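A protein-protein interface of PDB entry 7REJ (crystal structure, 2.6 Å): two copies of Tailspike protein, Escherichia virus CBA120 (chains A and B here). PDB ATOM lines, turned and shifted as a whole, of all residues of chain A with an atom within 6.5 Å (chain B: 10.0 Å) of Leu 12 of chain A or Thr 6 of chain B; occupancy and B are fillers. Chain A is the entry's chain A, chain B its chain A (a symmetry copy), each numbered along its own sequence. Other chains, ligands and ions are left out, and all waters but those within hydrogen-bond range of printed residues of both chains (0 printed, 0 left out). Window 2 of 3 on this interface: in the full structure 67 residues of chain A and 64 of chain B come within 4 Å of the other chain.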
ATOM      1  N   PHE A  10      -2.002  35.136 -15.022  1.00  0.00           N
ATOM      2  CA  PHE A  10      -3.237  34.782 -15.778  1.00  0.00           C
ATOM      3  C   PHE A  10      -4.421  34.907 -14.819  1.00  0.00           C
ATOM      4  O   PHE A  10      -4.844  33.938 -14.197  1.00  0.00           O
ATOM      5  CB  PHE A  10      -3.142  33.368 -16.350  1.00  0.00           C
ATOM      6  CG  PHE A  10      -2.142  33.190 -17.457  1.00  0.00           C
ATOM      7  CD1 PHE A  10      -0.795  33.169 -17.186  1.00  0.00           C
ATOM      8  CD2 PHE A  10      -2.558  33.043 -18.764  1.00  0.00           C
ATOM      9  CE1 PHE A  10       0.126  33.005 -18.203  1.00  0.00           C
ATOM     10  CE2 PHE A  10      -1.642  32.880 -19.782  1.00  0.00           C
ATOM     11  CZ  PHE A  10      -0.298  32.861 -19.500  1.00  0.00           C
ATOM     12  N   PRO A  11      -5.015  36.095 -14.646  1.00  0.00           N
ATOM     13  CA  PRO A  11      -6.061  36.289 -13.650  1.00  0.00           C
ATOM     14  C   PRO A  11      -7.343  35.457 -13.728  1.00  0.00           C
ATOM     15  O   PRO A  11      -8.025  35.381 -12.728  1.00  0.00           O
ATOM     16  CB  PRO A  11      -6.440  37.740 -13.827  1.00  0.00           C
ATOM     17  CG  PRO A  11      -5.171  38.328 -14.371  1.00  0.00           C
ATOM     18  CD  PRO A  11      -4.718  37.309 -15.384  1.00  0.00           C
ATOM     19  N   LEU A  12      -7.646  34.863 -14.870  1.00  0.00           N
ATOM     20  CA  LEU A  12      -8.851  34.000 -14.990  1.00  0.00           C
ATOM     21  C   LEU A  12      -8.424  32.543 -15.171  1.00  0.00           C
ATOM     22  O   LEU A  12      -9.233  31.715 -15.596  1.00  0.00           O
ATOM     23  CB  LEU A  12      -9.694  34.525 -16.152  1.00  0.00           C
ATOM     24  CG  LEU A  12     -10.158  35.959 -15.965  1.00  0.00           C
ATOM     25  CD1 LEU A  12     -10.963  36.421 -17.156  1.00  0.00           C
ATOM     26  CD2 LEU A  12     -10.971  36.104 -14.702  1.00  0.00           C
ATOM     27  N   GLY A  13      -7.178  32.254 -14.853  1.00  0.00           N
ATOM     28  CA  GLY A  13      -6.572  30.938 -15.141  1.00  0.00           C
ATOM     29  C   GLY A  13      -6.343  30.764 -16.630  1.00  0.00           C
ATOM     30  O   GLY A  13      -6.420  31.773 -17.327  1.00  0.00           O
ATOM     31  N   LEU A  14      -6.074  29.540 -17.080  1.00  0.00           N
ATOM     32  CA  LEU A  14      -5.860  29.215 -18.511  1.00  0.00           C
ATOM     33  C   LEU A  14      -6.488  27.857 -18.773  1.00  0.00           C
ATOM     34  O   LEU A  14      -6.461  27.050 -17.859  1.00  0.00           O
ATOM     35  CB  LEU A  14      -4.380  29.250 -18.891  1.00  0.00           C
ATOM     36  CG  LEU A  14      -3.418  28.418 -18.051  1.00  0.00           C
ATOM     37  CD1 LEU A  14      -3.227  27.037 -18.643  1.00  0.00           C
ATOM     38  CD2 LEU A  14      -2.056  29.110 -17.940  1.00  0.00           C
ATOM     39  N   GLU A  15      -7.024  27.648 -19.972  1.00  0.00           N
ATOM     40  CA  GLU A  15      -7.411  26.312 -20.466  1.00  0.00           C
ATOM     41  C   GLU A  15      -6.246  25.795 -21.307  1.00  0.00           C
ATOM     42  O   GLU A  15      -5.535  26.615 -21.875  1.00  0.00           O
ATOM     43  CB  GLU A  15      -8.740  26.326 -21.227  1.00  0.00           C
ATOM     44  CG  GLU A  15      -9.040  24.992 -21.868  1.00  0.00           C
ATOM     45  CD  GLU A  15     -10.314  24.954 -22.687  1.00  0.00           C
ATOM     46  OE1 GLU A  15     -11.201  25.795 -22.341  1.00  0.00           O
ATOM     47  OE2 GLU A  15     -10.414  24.085 -23.668  1.00  0.00           O
ATOM     48  N   LYS B   4     -17.948  34.366 -25.418  1.00  0.00           N
ATOM     49  CA  LYS B   4     -18.040  32.989 -24.822  1.00  0.00           C
ATOM     50  C   LYS B   4     -16.712  32.634 -24.135  1.00  0.00           C
ATOM     51  O   LYS B   4     -16.690  32.462 -22.920  1.00  0.00           O
ATOM     52  CB  LYS B   4     -18.524  31.995 -25.887  1.00  0.00           C
ATOM     53  N   PRO B   5     -15.566  32.507 -24.847  1.00  0.00           N
ATOM     54  CA  PRO B   5     -14.303  32.095 -24.216  1.00  0.00           C
ATOM     55  C   PRO B   5     -14.017  32.873 -22.919  1.00  0.00           C
ATOM     56  O   PRO B   5     -13.967  34.088 -22.893  1.00  0.00           O
ATOM     57  CB  PRO B   5     -13.233  32.325 -25.300  1.00  0.00           C
ATOM     58  CG  PRO B   5     -14.006  32.218 -26.599  1.00  0.00           C
ATOM     59  CD  PRO B   5     -15.400  32.745 -26.288  1.00  0.00           C
ATOM     60  N   THR B   6     -13.833  32.132 -21.840  1.00  0.00           N
ATOM     61  CA  THR B   6     -13.714  32.704 -20.467  1.00  0.00           C
ATOM     62  C   THR B   6     -12.250  33.037 -20.172  1.00  0.00           C
ATOM     63  O   THR B   6     -11.986  33.978 -19.394  1.00  0.00           O
ATOM     64  CB  THR B   6     -14.344  31.756 -19.428  1.00  0.00           C
ATOM     65  OG1 THR B   6     -13.759  30.447 -19.464  1.00  0.00           O
ATOM     66  CG2 THR B   6     -15.842  31.620 -19.615  1.00  0.00           C
ATOM     67  N   GLN B   7     -11.329  32.292 -20.770  1.00  0.00           N
ATOM     68  CA  GLN B   7      -9.903  32.482 -20.452  1.00  0.00           C
ATOM     69  C   GLN B   7      -9.032  32.025 -21.606  1.00  0.00           C
ATOM     70  O   GLN B   7      -9.521  31.368 -22.521  1.00  0.00           O
ATOM     71  CB  GLN B   7      -9.585  31.666 -19.197  1.00  0.00           C
ATOM     72  CG  GLN B   7      -9.500  30.177 -19.467  1.00  0.00           C
ATOM     73  CD  GLN B   7     -10.090  29.319 -18.371  1.00  0.00           C
ATOM     74  OE1 GLN B   7     -10.177  29.727 -17.215  1.00  0.00           O
ATOM     75  NE2 GLN B   7     -10.500  28.108 -18.738  1.00  0.00           N
ATOM     76  N   PRO B   8      -7.733  32.373 -21.564  1.00  0.00           N
ATOM     77  CA  PRO B   8      -6.787  32.008 -22.602  1.00  0.00           C
ATOM     78  C   PRO B   8      -6.721  30.521 -22.879  1.00  0.00           C
ATOM     79  O   PRO B   8      -6.693  29.816 -21.972  1.00  0.00           O
ATOM     80  CB  PRO B   8      -5.427  32.451 -22.059  1.00  0.00           C
ATOM     81  CG  PRO B   8      -5.798  33.621 -21.173  1.00  0.00           C
ATOM     82  CD  PRO B   8      -7.076  33.148 -20.515  1.00  0.00           C
ATOM     83  N   LEU B   9      -6.700  30.162 -24.142  1.00  0.00           N
ATOM     84  CA  LEU B   9      -6.663  28.764 -24.590  1.00  0.00           C
ATOM     85  C   LEU B   9      -5.281  28.468 -25.178  1.00  0.00           C
ATOM     86  O   LEU B   9      -4.798  29.221 -25.993  1.00  0.00           O
ATOM     87  CB  LEU B   9      -7.775  28.587 -25.627  1.00  0.00           C
ATOM     88  CG  LEU B   9      -7.730  27.271 -26.396  1.00  0.00           C
ATOM     89  CD1 LEU B   9      -7.692  26.093 -25.437  1.00  0.00           C
ATOM     90  CD2 LEU B   9      -8.929  27.164 -27.317  1.00  0.00           C
ATOM     91  N   PHE B  10      -4.667  27.387 -24.763  1.00  0.00           N
ATOM     92  CA  PHE B  10      -3.339  26.918 -25.257  1.00  0.00           C
ATOM     93  C   PHE B  10      -3.546  25.561 -25.929  1.00  0.00           C
ATOM     94  O   PHE B  10      -3.390  24.512 -25.312  1.00  0.00           O
ATOM     95  CB  PHE B  10      -2.335  26.814 -24.110  1.00  0.00           C
ATOM     96  CG  PHE B  10      -1.904  28.124 -23.515  1.00  0.00           C
ATOM     97  CD1 PHE B  10      -2.754  28.838 -22.704  1.00  0.00           C
ATOM     98  CD2 PHE B  10      -0.647  28.634 -23.771  1.00  0.00           C
ATOM     99  CE1 PHE B  10      -2.358  30.043 -22.155  1.00  0.00           C
ATOM    100  CE2 PHE B  10      -0.249  29.836 -23.225  1.00  0.00           C
ATOM    101  CZ  PHE B  10      -1.107  30.541 -22.417  1.00  0.00           C
ATOM    102  N   ILE B  22      -0.129  28.089  -9.044  1.00  0.00           N
ATOM    103  CA  ILE B  22      -1.449  27.851  -9.678  1.00  0.00           C
ATOM    104  C   ILE B  22      -2.533  27.752  -8.625  1.00  0.00           C
ATOM    105  O   ILE B  22      -2.386  26.916  -7.768  1.00  0.00           O
ATOM    106  CB  ILE B  22      -1.300  26.557 -10.449  1.00  0.00           C
ATOM    107  CG1 ILE B  22       0.013  26.659 -11.233  1.00  0.00           C
ATOM    108  CG2 ILE B  22      -2.544  26.304 -11.289  1.00  0.00           C
ATOM    109  CD1 ILE B  22       0.205  25.612 -12.319  1.00  0.00           C
ATOM    110  N   LYS B  23      -3.566  28.576  -8.701  1.00  0.00           N
ATOM    111  CA  LYS B  23      -4.748  28.462  -7.807  1.00  0.00           C
ATOM    112  C   LYS B  23      -5.692  27.413  -8.402  1.00  0.00           C
ATOM    113  O   LYS B  23      -6.814  27.726  -8.799  1.00  0.00           O
ATOM    114  CB  LYS B  23      -5.404  29.820  -7.543  1.00  0.00           C
ATOM    115  CG  LYS B  23      -6.808  29.750  -6.951  1.00  0.00           C
ATOM    116  CD  LYS B  23      -7.188  30.868  -5.986  1.00  0.00           C
ATOM    117  CE  LYS B  23      -8.675  30.892  -5.688  1.00  0.00           C
ATOM    118  NZ  LYS B  23      -9.035  31.929  -4.690  1.00  0.00           N
ATOM    119  N   GLY B  24      -5.225  26.183  -8.457  1.00  0.00           N
ATOM    120  CA  GLY B  24      -6.053  24.996  -8.723  1.00  0.00           C
ATOM    121  C   GLY B  24      -6.396  24.807 -10.191  1.00  0.00           C
ATOM    122  O   GLY B  24      -6.197  25.746 -10.970  1.00  0.00           O
ATOM    123  N   PHE B  25      -6.896  23.617 -10.530  1.00  0.00           N
ATOM    124  CA  PHE B  25      -7.475  23.318 -11.857  1.00  0.00           C
ATOM    125  C   PHE B  25      -8.341  22.061 -11.917  1.00  0.00           C
ATOM    126  O   PHE B  25      -7.950  21.040 -11.322  1.00  0.00           O
ATOM    127  CB  PHE B  25      -6.348  23.005 -12.821  1.00  0.00           C
ATOM    128  CG  PHE B  25      -5.366  21.998 -12.303  1.00  0.00           C
ATOM    129  CD1 PHE B  25      -4.274  22.416 -11.568  1.00  0.00           C
ATOM    130  CD2 PHE B  25      -5.536  20.648 -12.549  1.00  0.00           C
ATOM    131  CE1 PHE B  25      -3.350  21.494 -11.079  1.00  0.00           C
ATOM    132  CE2 PHE B  25      -4.616  19.725 -12.062  1.00  0.00           C
ATOM    133  CZ  PHE B  25      -3.523  20.149 -11.327  1.00  0.00           C
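OE1 of Gln 7 of chain B lies close to O of Leu 12 of chain A, 2.7 Å away.
N of Glu 15 of chain A lies within hydrogen-bond range of O of Pro 8 of chain B (3.0 Å).
O of Glu 15 of chain A lies within hydrogen-bond range of N of Phe 10 of chain B.
Phe 10 of chain B touches Phe 10 of chain A (CZ to CE2, 3.6 Å).
Leu 12 of chain A touches Thr 6 of chain B.
O of Gly 13 of chain A touches CB of Gln 7 of chain B (3.7 Å).
CD of Pro 8 of chain B touches O of Gly 13 of chain A, 3.5 Å away.
Leu 14 of chain A touches Gln 7 of chain B.
Leu 14 of chain A touches Pro 8 of chain B (CA to O, 3.6 Å).
Leu 14 of chain A touches Phe 10 of chain B.
Glu 15 of chain A touches Gln 7 of chain B.
O of Glu 15 of chain A touches CA of Leu 9 of chain B, 3.6 Å away.
Of chain B, only Thr 6 and Gln 7 come within 4 Å of Leu 12 of chain A.
No residue of chain B comes within 4 Å of Pro 11 of chain A.
Gly 13 of chain A touches just these residues of chain B: Gln 7 and Pro 8.
Printed residues of chain B within 4 Å of Phe 10 of chain A: Phe 10 (3.6 Å).
Of the printed residues of chain B, Glu 15 of chain A touches Gln 7 (3.5 Å), Pro 8 (3.0 Å), Leu 9 (3.6 Å) and Phe 10 (3.1 Å).
Of the printed residues of chain B, Leu 14 of chain A touches Gln 7, Pro 8 and Phe 10.
Of the printed residues of chain A, Phe 10 of chain B touches Phe 10 (3.6 Å), Leu 14 (3.9 Å) and Glu 15 (3.1 Å).
Printed residues of chain A within 4 Å of Gln 7 of chain B: Leu 12 (2.7 Å), Gly 13 (3.7 Å), Leu 14 (3.9 Å) and Glu 15 (3.5 Å).
Phe 25 of chain B touches none of the printed residues of chain A.
Gly 24 of chain B touches none of the printed residues of chain A.
The nearest printed residue of chain B that does not touch Glu 15 of chain A is Thr 6 of chain B (6.0 Å).
Printed residues of chain A that touch a printed residue of chain B: Phe 10, Leu 12, Gly 13, Leu 14 and Glu 15.
Of the 11 printed residues of chain B, 5 touch a printed residue of chain A.
Phe 10 of chain A touches its own counterpart, Phe 10 of chain B.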
